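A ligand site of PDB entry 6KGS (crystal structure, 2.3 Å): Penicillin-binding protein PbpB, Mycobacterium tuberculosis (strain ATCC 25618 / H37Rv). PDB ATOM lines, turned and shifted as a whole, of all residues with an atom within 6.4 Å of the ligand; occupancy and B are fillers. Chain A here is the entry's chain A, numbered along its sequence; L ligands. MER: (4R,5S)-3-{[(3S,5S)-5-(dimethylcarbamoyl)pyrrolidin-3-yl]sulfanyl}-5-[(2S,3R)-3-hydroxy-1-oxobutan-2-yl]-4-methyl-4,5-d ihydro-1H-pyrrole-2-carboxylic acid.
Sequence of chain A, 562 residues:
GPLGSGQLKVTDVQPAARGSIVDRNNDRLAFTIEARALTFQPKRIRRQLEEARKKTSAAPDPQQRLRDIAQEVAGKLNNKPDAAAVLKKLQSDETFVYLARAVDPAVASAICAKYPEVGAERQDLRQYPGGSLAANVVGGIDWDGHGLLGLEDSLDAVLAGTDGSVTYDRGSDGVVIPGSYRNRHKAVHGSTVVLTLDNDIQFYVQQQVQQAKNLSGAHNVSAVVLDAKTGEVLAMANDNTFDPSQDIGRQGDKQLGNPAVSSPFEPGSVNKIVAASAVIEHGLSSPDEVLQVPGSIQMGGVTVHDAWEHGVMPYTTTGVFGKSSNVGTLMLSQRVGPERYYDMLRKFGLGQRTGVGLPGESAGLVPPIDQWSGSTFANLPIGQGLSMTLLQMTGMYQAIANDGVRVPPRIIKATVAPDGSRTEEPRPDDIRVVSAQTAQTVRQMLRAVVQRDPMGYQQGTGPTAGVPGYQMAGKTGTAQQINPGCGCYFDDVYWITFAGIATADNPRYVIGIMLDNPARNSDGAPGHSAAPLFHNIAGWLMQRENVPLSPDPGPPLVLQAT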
ATOM      1  N   PRO A 267      20.882 -12.981 -22.169  1.00  0.00           N
ATOM      2  CA  PRO A 267      20.654 -11.551 -21.872  1.00  0.00           C
ATOM      3  C   PRO A 267      20.639 -10.638 -23.089  1.00  0.00           C
ATOM      4  O   PRO A 267      20.112  -9.518 -22.994  1.00  0.00           O
ATOM      5  CB  PRO A 267      21.824 -11.206 -20.962  1.00  0.00           C
ATOM      6  CG  PRO A 267      22.962 -12.146 -21.533  1.00  0.00           C
ATOM      7  CD  PRO A 267      22.214 -13.424 -21.720  1.00  0.00           C
ATOM      8  N   GLY A 268      21.216 -11.054 -24.210  1.00  0.00           N
ATOM      9  CA  GLY A 268      21.351 -10.144 -25.321  1.00  0.00           C
ATOM     10  C   GLY A 268      22.304  -9.006 -24.969  1.00  0.00           C
ATOM     11  O   GLY A 268      23.199  -9.140 -24.137  1.00  0.00           O
ATOM     12  N   SER A 269      22.076  -7.861 -25.617  1.00  0.00           N
ATOM     13  CA  SER A 269      23.043  -6.751 -25.562  1.00  0.00           C
ATOM     14  C   SER A 269      23.208  -6.143 -24.163  1.00  0.00           C
ATOM     15  O   SER A 269      24.172  -5.382 -23.951  1.00  0.00           O
ATOM     16  CB  SER A 269      22.608  -5.669 -26.537  1.00  0.00           C
ATOM     17  OG  SER A 269      22.565  -6.197 -27.834  1.00  0.00           O
ATOM     18  N   VAL A 270      22.319  -6.443 -23.225  1.00  0.00           N
ATOM     19  CA  VAL A 270      22.561  -6.033 -21.832  1.00  0.00           C
ATOM     20  C   VAL A 270      23.885  -6.605 -21.332  1.00  0.00           C
ATOM     21  O   VAL A 270      24.560  -5.990 -20.503  1.00  0.00           O
ATOM     22  CB  VAL A 270      21.354  -6.424 -20.959  1.00  0.00           C
ATOM     23  CG1 VAL A 270      21.660  -6.283 -19.481  1.00  0.00           C
ATOM     24  CG2 VAL A 270      20.162  -5.520 -21.297  1.00  0.00           C
ATOM     25  N   LYS A 272      26.561  -6.386 -22.790  1.00  0.00           N
ATOM     26  CA  LYS A 272      27.712  -5.677 -23.311  1.00  0.00           C
ATOM     27  C   LYS A 272      28.407  -4.828 -22.260  1.00  0.00           C
ATOM     28  O   LYS A 272      29.490  -4.306 -22.523  1.00  0.00           O
ATOM     29  CB  LYS A 272      27.292  -4.818 -24.506  1.00  0.00           C
ATOM     30  CG  LYS A 272      26.878  -5.647 -25.719  1.00  0.00           C
ATOM     31  CD  LYS A 272      26.439  -4.745 -26.874  1.00  0.00           C
ATOM     32  CE  LYS A 272      25.959  -5.546 -28.077  1.00  0.00           C
ATOM     33  NZ  LYS A 272      25.589  -4.645 -29.219  1.00  0.00           N
ATOM     34  N   HIS A 305      26.508  -9.319 -37.822  1.00  0.00           N
ATOM     35  CA  HIS A 305      25.925  -8.198 -38.530  1.00  0.00           C
ATOM     36  C   HIS A 305      25.331  -7.237 -37.502  1.00  0.00           C
ATOM     37  O   HIS A 305      24.901  -7.659 -36.430  1.00  0.00           O
ATOM     38  CB  HIS A 305      24.837  -8.711 -39.464  1.00  0.00           C
ATOM     39  CG  HIS A 305      24.620  -7.857 -40.669  1.00  0.00           C
ATOM     40  ND1 HIS A 305      24.895  -8.309 -41.945  1.00  0.00           N
ATOM     41  CD2 HIS A 305      24.146  -6.598 -40.802  1.00  0.00           C
ATOM     42  CE1 HIS A 305      24.621  -7.352 -42.806  1.00  0.00           C
ATOM     43  NE2 HIS A 305      24.158  -6.312 -42.144  1.00  0.00           N
ATOM     44  N   ASP A 306      25.330  -5.941 -37.810  1.00  0.00           N
ATOM     45  CA  ASP A 306      24.610  -5.001 -36.960  1.00  0.00           C
ATOM     46  C   ASP A 306      23.127  -5.001 -37.317  1.00  0.00           C
ATOM     47  O   ASP A 306      22.750  -5.195 -38.471  1.00  0.00           O
ATOM     48  CB  ASP A 306      25.182  -3.584 -37.099  1.00  0.00           C
ATOM     49  CG  ASP A 306      26.418  -3.369 -36.238  1.00  0.00           C
ATOM     50  OD1 ASP A 306      26.774  -4.272 -35.465  1.00  0.00           O
ATOM     51  OD2 ASP A 306      27.038  -2.284 -36.305  1.00  0.00           O
ATOM     52  N   ALA A 307      22.278  -4.768 -36.301  1.00  0.00           N
ATOM     53  CA  ALA A 307      20.813  -4.771 -36.425  1.00  0.00           C
ATOM     54  C   ALA A 307      20.269  -3.871 -37.534  1.00  0.00           C
ATOM     55  O   ALA A 307      19.066  -3.930 -37.852  1.00  0.00           O
ATOM     56  CB  ALA A 307      20.164  -4.357 -35.111  1.00  0.00           C
ATOM     57  N   TRP A 308      21.111  -3.006 -38.089  1.00  0.00           N
ATOM     58  CA  TRP A 308      20.761  -2.155 -39.209  1.00  0.00           C
ATOM     59  C   TRP A 308      21.884  -2.258 -40.230  1.00  0.00           C
ATOM     60  O   TRP A 308      23.054  -2.436 -39.873  1.00  0.00           O
ATOM     61  CB  TRP A 308      20.525  -0.679 -38.761  1.00  0.00           C
ATOM     62  CG  TRP A 308      21.725   0.035 -38.105  1.00  0.00           C
ATOM     63  CD1 TRP A 308      22.398   1.125 -38.598  1.00  0.00           C
ATOM     64  CD2 TRP A 308      22.366  -0.291 -36.845  1.00  0.00           C
ATOM     65  NE1 TRP A 308      23.417   1.481 -37.733  1.00  0.00           N
ATOM     66  CE2 TRP A 308      23.420   0.639 -36.651  1.00  0.00           C
ATOM     67  CE3 TRP A 308      22.161  -1.273 -35.858  1.00  0.00           C
ATOM     68  CZ2 TRP A 308      24.267   0.609 -35.529  1.00  0.00           C
ATOM     69  CZ3 TRP A 308      23.000  -1.297 -34.734  1.00  0.00           C
ATOM     70  CH2 TRP A 308      24.036  -0.370 -34.587  1.00  0.00           C
ATOM     71  N   LYS A 323      24.453   2.893 -29.355  1.00  0.00           N
ATOM     72  CA  LYS A 323      23.678   2.387 -30.480  1.00  0.00           C
ATOM     73  C   LYS A 323      23.593   0.871 -30.511  1.00  0.00           C
ATOM     74  O   LYS A 323      22.909   0.323 -31.373  1.00  0.00           O
ATOM     75  CB  LYS A 323      24.279   2.907 -31.802  1.00  0.00           C
ATOM     76  CG  LYS A 323      23.875   4.363 -32.080  1.00  0.00           C
ATOM     77  CD  LYS A 323      24.545   4.982 -33.266  1.00  0.00           C
ATOM     78  CE  LYS A 323      24.312   6.498 -33.280  1.00  0.00           C
ATOM     79  NZ  LYS A 323      22.864   6.948 -33.286  1.00  0.00           N
ATOM     80  N   SER A 324      24.276   0.188 -29.593  1.00  0.00           N
ATOM     81  CA  SER A 324      24.340  -1.268 -29.510  1.00  0.00           C
ATOM     82  C   SER A 324      24.807  -1.909 -30.830  1.00  0.00           C
ATOM     83  O   SER A 324      24.149  -2.789 -31.397  1.00  0.00           O
ATOM     84  CB  SER A 324      22.988  -1.842 -29.051  1.00  0.00           C
ATOM     85  OG  SER A 324      23.185  -3.137 -28.501  1.00  0.00           O
ATOM     86  N   SER A 325      25.996  -1.513 -31.275  1.00  0.00           N
ATOM     87  CA  SER A 325      26.632  -2.116 -32.447  1.00  0.00           C
ATOM     88  C   SER A 325      27.316  -3.437 -32.082  1.00  0.00           C
ATOM     89  O   SER A 325      28.196  -3.455 -31.216  1.00  0.00           O
ATOM     90  CB  SER A 325      27.637  -1.154 -33.065  1.00  0.00           C
ATOM     91  OG  SER A 325      28.468  -1.797 -34.020  1.00  0.00           O
ATOM     92  N   ASN A 326      26.885  -4.535 -32.714  1.00  0.00           N
ATOM     93  CA  ASN A 326      27.526  -5.837 -32.492  1.00  0.00           C
ATOM     94  C   ASN A 326      28.945  -5.854 -33.040  1.00  0.00           C
ATOM     95  O   ASN A 326      29.872  -6.358 -32.384  1.00  0.00           O
ATOM     96  CB  ASN A 326      26.703  -6.953 -33.152  1.00  0.00           C
ATOM     97  CG  ASN A 326      25.377  -7.184 -32.473  1.00  0.00           C
ATOM     98  OD1 ASN A 326      25.202  -6.845 -31.304  1.00  0.00           O
ATOM     99  ND2 ASN A 326      24.426  -7.769 -33.210  1.00  0.00           N
ATOM    100  N   ILE A 382      28.100 -10.218 -27.078  1.00  0.00           N
ATOM    101  CA  ILE A 382      26.828  -9.554 -27.397  1.00  0.00           C
ATOM    102  C   ILE A 382      25.650 -10.183 -26.665  1.00  0.00           C
ATOM    103  O   ILE A 382      24.497  -9.750 -26.859  1.00  0.00           O
ATOM    104  CB  ILE A 382      26.563  -9.542 -28.923  1.00  0.00           C
ATOM    105  CG1 ILE A 382      26.290 -10.965 -29.447  1.00  0.00           C
ATOM    106  CG2 ILE A 382      27.743  -8.863 -29.650  1.00  0.00           C
ATOM    107  CD1 ILE A 382      26.022 -11.026 -30.968  1.00  0.00           C
ATOM    108  N   GLY A 383      25.899 -11.145 -25.789  1.00  0.00           N
ATOM    109  CA  GLY A 383      24.887 -11.672 -24.914  1.00  0.00           C
ATOM    110  C   GLY A 383      24.160 -12.907 -25.391  1.00  0.00           C
ATOM    111  O   GLY A 383      23.109 -13.222 -24.839  1.00  0.00           O
ATOM    112  N   GLN A 384      24.676 -13.630 -26.390  1.00  0.00           N
ATOM    113  CA  GLN A 384      24.112 -14.919 -26.799  1.00  0.00           C
ATOM    114  C   GLN A 384      25.104 -16.020 -26.428  1.00  0.00           C
ATOM    115  O   GLN A 384      26.309 -15.787 -26.374  1.00  0.00           O
ATOM    116  CB  GLN A 384      23.809 -14.977 -28.311  1.00  0.00           C
ATOM    117  CG  GLN A 384      22.705 -13.994 -28.819  1.00  0.00           C
ATOM    118  CD  GLN A 384      21.213 -14.451 -28.760  1.00  0.00           C
ATOM    119  OE1 GLN A 384      20.765 -15.303 -27.949  1.00  0.00           O
ATOM    120  NE2 GLN A 384      20.427 -13.795 -29.603  1.00  0.00           N
ATOM    121  N   THR A 461      19.672   3.695 -28.247  1.00  0.00           N
ATOM    122  CA  THR A 461      18.599   2.747 -28.500  1.00  0.00           C
ATOM    123  C   THR A 461      17.443   2.834 -27.504  1.00  0.00           C
ATOM    124  O   THR A 461      16.379   2.270 -27.777  1.00  0.00           O
ATOM    125  CB  THR A 461      19.136   1.314 -28.481  1.00  0.00           C
ATOM    126  OG1 THR A 461      19.699   1.053 -27.175  1.00  0.00           O
ATOM    127  CG2 THR A 461      20.204   1.080 -29.593  1.00  0.00           C
ATOM    128  N   LYS A 475      21.002   0.016 -20.393  1.00  0.00           N
ATOM    129  CA  LYS A 475      21.323  -0.731 -21.614  1.00  0.00           C
ATOM    130  C   LYS A 475      20.107  -1.570 -22.008  1.00  0.00           C
ATOM    131  O   LYS A 475      19.475  -2.176 -21.151  1.00  0.00           O
ATOM    132  CB  LYS A 475      22.576  -1.619 -21.413  1.00  0.00           C
ATOM    133  CG  LYS A 475      23.044  -2.358 -22.690  1.00  0.00           C
ATOM    134  CD  LYS A 475      23.529  -1.358 -23.755  1.00  0.00           C
ATOM    135  CE  LYS A 475      23.860  -2.012 -25.095  1.00  0.00           C
ATOM    136  NZ  LYS A 475      22.608  -2.244 -25.881  1.00  0.00           N
ATOM    137  N   THR A 476      19.798  -1.567 -23.317  1.00  0.00           N
ATOM    138  CA  THR A 476      18.710  -2.348 -23.914  1.00  0.00           C
ATOM    139  C   THR A 476      19.216  -3.715 -24.367  1.00  0.00           C
ATOM    140  O   THR A 476      20.397  -3.879 -24.673  1.00  0.00           O
ATOM    141  CB  THR A 476      18.113  -1.621 -25.128  1.00  0.00           C
ATOM    142  OG1 THR A 476      19.195  -1.169 -25.966  1.00  0.00           O
ATOM    143  CG2 THR A 476      17.255  -0.390 -24.693  1.00  0.00           C
ATOM    144  N   GLY A 477      18.306  -4.680 -24.434  1.00  0.00           N
ATOM    145  CA  GLY A 477      18.662  -5.987 -24.928  1.00  0.00           C
ATOM    146  C   GLY A 477      17.520  -6.698 -25.619  1.00  0.00           C
ATOM    147  O   GLY A 477      16.346  -6.584 -25.246  1.00  0.00           O
ATOM    148  N   THR A 478      17.886  -7.485 -26.637  1.00  0.00           N
ATOM    149  CA  THR A 478      17.001  -8.372 -27.366  1.00  0.00           C
ATOM    150  C   THR A 478      17.809  -9.638 -27.657  1.00  0.00           C
ATOM    151  O   THR A 478      18.895  -9.554 -28.228  1.00  0.00           O
ATOM    152  CB  THR A 478      16.517  -7.729 -28.678  1.00  0.00           C
ATOM    153  OG1 THR A 478      15.859  -6.488 -28.384  1.00  0.00           O
ATOM    154  CG2 THR A 478      15.551  -8.643 -29.420  1.00  0.00           C
ATOM    155  N   ALA A 479      17.296 -10.796 -27.240  1.00  0.00           N
ATOM    156  CA  ALA A 479      18.009 -12.055 -27.435  1.00  0.00           C
ATOM    157  C   ALA A 479      17.046 -13.102 -27.962  1.00  0.00           C
ATOM    158  O   ALA A 479      15.960 -13.301 -27.401  1.00  0.00           O
ATOM    159  CB  ALA A 479      18.674 -12.534 -26.132  1.00  0.00           C
ATOM    160  N   TYR A 494      11.926 -13.608 -28.748  1.00  0.00           N
ATOM    161  CA  TYR A 494      12.990 -12.923 -28.030  1.00  0.00           C
ATOM    162  C   TYR A 494      12.666 -12.742 -26.558  1.00  0.00           C
ATOM    163  O   TYR A 494      11.507 -12.636 -26.159  1.00  0.00           O
ATOM    164  CB  TYR A 494      13.280 -11.535 -28.609  1.00  0.00           C
ATOM    165  CG  TYR A 494      13.395 -11.471 -30.110  1.00  0.00           C
ATOM    166  CD1 TYR A 494      14.591 -11.744 -30.760  1.00  0.00           C
ATOM    167  CD2 TYR A 494      12.284 -11.115 -30.889  1.00  0.00           C
ATOM    168  CE1 TYR A 494      14.694 -11.658 -32.143  1.00  0.00           C
ATOM    169  CE2 TYR A 494      12.378 -11.037 -32.281  1.00  0.00           C
ATOM    170  CZ  TYR A 494      13.582 -11.313 -32.902  1.00  0.00           C
ATOM    171  OH  TYR A 494      13.679 -11.222 -34.273  1.00  0.00           O
ATOM    172  N   THR A 497      15.212  -7.194 -22.601  1.00  0.00           N
ATOM    173  CA  THR A 497      15.880  -6.909 -21.334  1.00  0.00           C
ATOM    174  C   THR A 497      16.232  -5.440 -21.260  1.00  0.00           C
ATOM    175  O   THR A 497      16.437  -4.777 -22.275  1.00  0.00           O
ATOM    176  CB  THR A 497      17.197  -7.723 -21.163  1.00  0.00           C
ATOM    177  OG1 THR A 497      18.029  -7.527 -22.313  1.00  0.00           O
ATOM    178  CG2 THR A 497      16.929  -9.218 -20.992  1.00  0.00           C
ATOM    179  N   GLY A 527       6.475  -1.780 -30.993  1.00  0.00           N
ATOM    180  CA  GLY A 527       7.870  -2.104 -30.767  1.00  0.00           C
ATOM    181  C   GLY A 527       7.964  -3.266 -29.797  1.00  0.00           C
ATOM    182  O   GLY A 527       7.026  -4.020 -29.611  1.00  0.00           O
ATOM    183  N   HIS A 528       9.122  -3.420 -29.166  1.00  0.00           N
ATOM    184  CA  HIS A 528       9.222  -4.426 -28.112  1.00  0.00           C
ATOM    185  C   HIS A 528      10.389  -4.090 -27.192  1.00  0.00           C
ATOM    186  O   HIS A 528      11.376  -4.823 -27.098  1.00  0.00           O
ATOM    187  CB  HIS A 528       9.298  -5.832 -28.700  1.00  0.00           C
ATOM    188  CG  HIS A 528      10.467  -6.045 -29.587  1.00  0.00           C
ATOM    189  ND1 HIS A 528      11.032  -5.024 -30.329  1.00  0.00           N
ATOM    190  CD2 HIS A 528      11.156  -7.172 -29.899  1.00  0.00           C
ATOM    191  CE1 HIS A 528      12.054  -5.493 -30.995  1.00  0.00           C
ATOM    192  NE2 HIS A 528      12.144  -6.804 -30.782  1.00  0.00           N
HETATM  193  C1  MER L   1      21.342  -6.691 -28.496  1.00  0.00           C
HETATM  194  C2  MER L   1      19.430  -4.610 -31.023  1.00  0.00           C
HETATM  195  C3  MER L   1      21.342  -6.968 -29.999  1.00  0.00           C
HETATM  196  C4  MER L   1      21.511  -5.662 -30.793  1.00  0.00           C
HETATM  197  C5  MER L   1      20.063  -4.034 -30.022  1.00  0.00           C
HETATM  198  O6  MER L   1      20.371  -6.874 -27.776  1.00  0.00           O
HETATM  199  C7  MER L   1      22.442  -7.996 -30.342  1.00  0.00           C
HETATM  200  O8  MER L   1      22.404  -8.371 -31.720  1.00  0.00           O
HETATM  201  C9  MER L   1      22.341  -9.290 -29.532  1.00  0.00           C
HETATM  202  N10 MER L   1      21.373  -4.492 -29.890  1.00  0.00           N
HETATM  203  C11 MER L   1      19.481  -3.053 -29.088  1.00  0.00           C
HETATM  204  O12 MER L   1      20.020  -2.953 -27.889  1.00  0.00           O
HETATM  205  O13 MER L   1      18.529  -2.322 -29.315  1.00  0.00           O
HETATM  206  S14 MER L   1      17.775  -4.498 -31.328  1.00  0.00           S
HETATM  207  C15 MER L   1      17.391  -3.005 -32.217  1.00  0.00           C
HETATM  208  C16 MER L   1      16.822  -3.339 -33.585  1.00  0.00           C
HETATM  209  C17 MER L   1      15.390  -2.803 -33.628  1.00  0.00           C
HETATM  210  C18 MER L   1      20.403  -5.398 -31.830  1.00  0.00           C
HETATM  211  N19 MER L   1      15.006  -2.557 -32.219  1.00  0.00           N
HETATM  212  C20 MER L   1      19.745  -6.654 -32.368  1.00  0.00           C
HETATM  213  C21 MER L   1      16.282  -2.203 -31.541  1.00  0.00           C
HETATM  214  C22 MER L   1      14.537  -3.791 -34.373  1.00  0.00           C
HETATM  215  N23 MER L   1      13.454  -4.384 -33.807  1.00  0.00           N
HETATM  216  O24 MER L   1      14.865  -3.994 -35.527  1.00  0.00           O
HETATM  217  C25 MER L   1      12.255  -3.632 -33.454  1.00  0.00           C
HETATM  218  C26 MER L   1      13.368  -5.813 -33.602  1.00  0.00           C
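The backbone NH (N) of Thr 478 sits at hydrogen-bond distance from an oxygen (O6) of the ligand. An oxygen (O12) of the ligand is in salt-bridge range of the side-chain amino group (NZ) of Lys 475 (3.4 Å). A carbon (C1) of the ligand is covalently linked to the side-chain hydroxyl (OG) of Ser 269, 1.5 Å away. OG1 of Thr 476 sits at hydrogen-bond distance from O12 of the ligand. The side-chain hydroxyl (OG) of Ser 324 sits at hydrogen-bond distance from a nitrogen (N10) of the ligand, at 2.7 Å. An oxygen (O6) of the ligand lies close to the backbone NH (N) of Ser 269. An oxygen (O8) of the ligand sits at hydrogen-bond distance from the side-chain amide nitrogen (ND2) of Asn 326 (2.6 Å).
Merely in contact with the ligand: Ala 307, Ile 382, Thr 461, Gly 477 and His 528. Within 4 Å of the ligand: Ser 269, Ala 307, Ser 324, Asn 326, Ile 382, Thr 461, Lys 475, Thr 476, Gly 477, Thr 478 and His 528.
The side-chain hydroxyl (OG) of Ser 269 sits at hydrogen-bond distance from the side-chain hydroxyl (OG) of Ser 324, at 3.2 Å. The side-chain carboxylate of Asp 306 sits at hydrogen-bond distance from the backbone NH of Asn 326, 2.8 Å away. NZ of Lys 272 lies within hydrogen-bond range of OD1 of Asn 326, at 3.1 Å. The side-chain hydroxyl of Thr 461 is in hydrogen-bond range of the side-chain hydroxyl of Thr 476, at 2.6 Å. The backbone NH (N) of Gly 477 lies within hydrogen-bond range of the backbone carbonyl oxygen (O) of Thr 497. The side-chain amino group (NZ) of Lys 272 sits at hydrogen-bond distance from the side-chain hydroxyl (OG) of Ser 324 (2.9 Å). The side-chain amino group of Lys 475 is in hydrogen-bond range of the side-chain hydroxyl of Ser 324 (2.8 Å). O of Ile 382 sits at hydrogen-bond distance from N of Ser 269.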
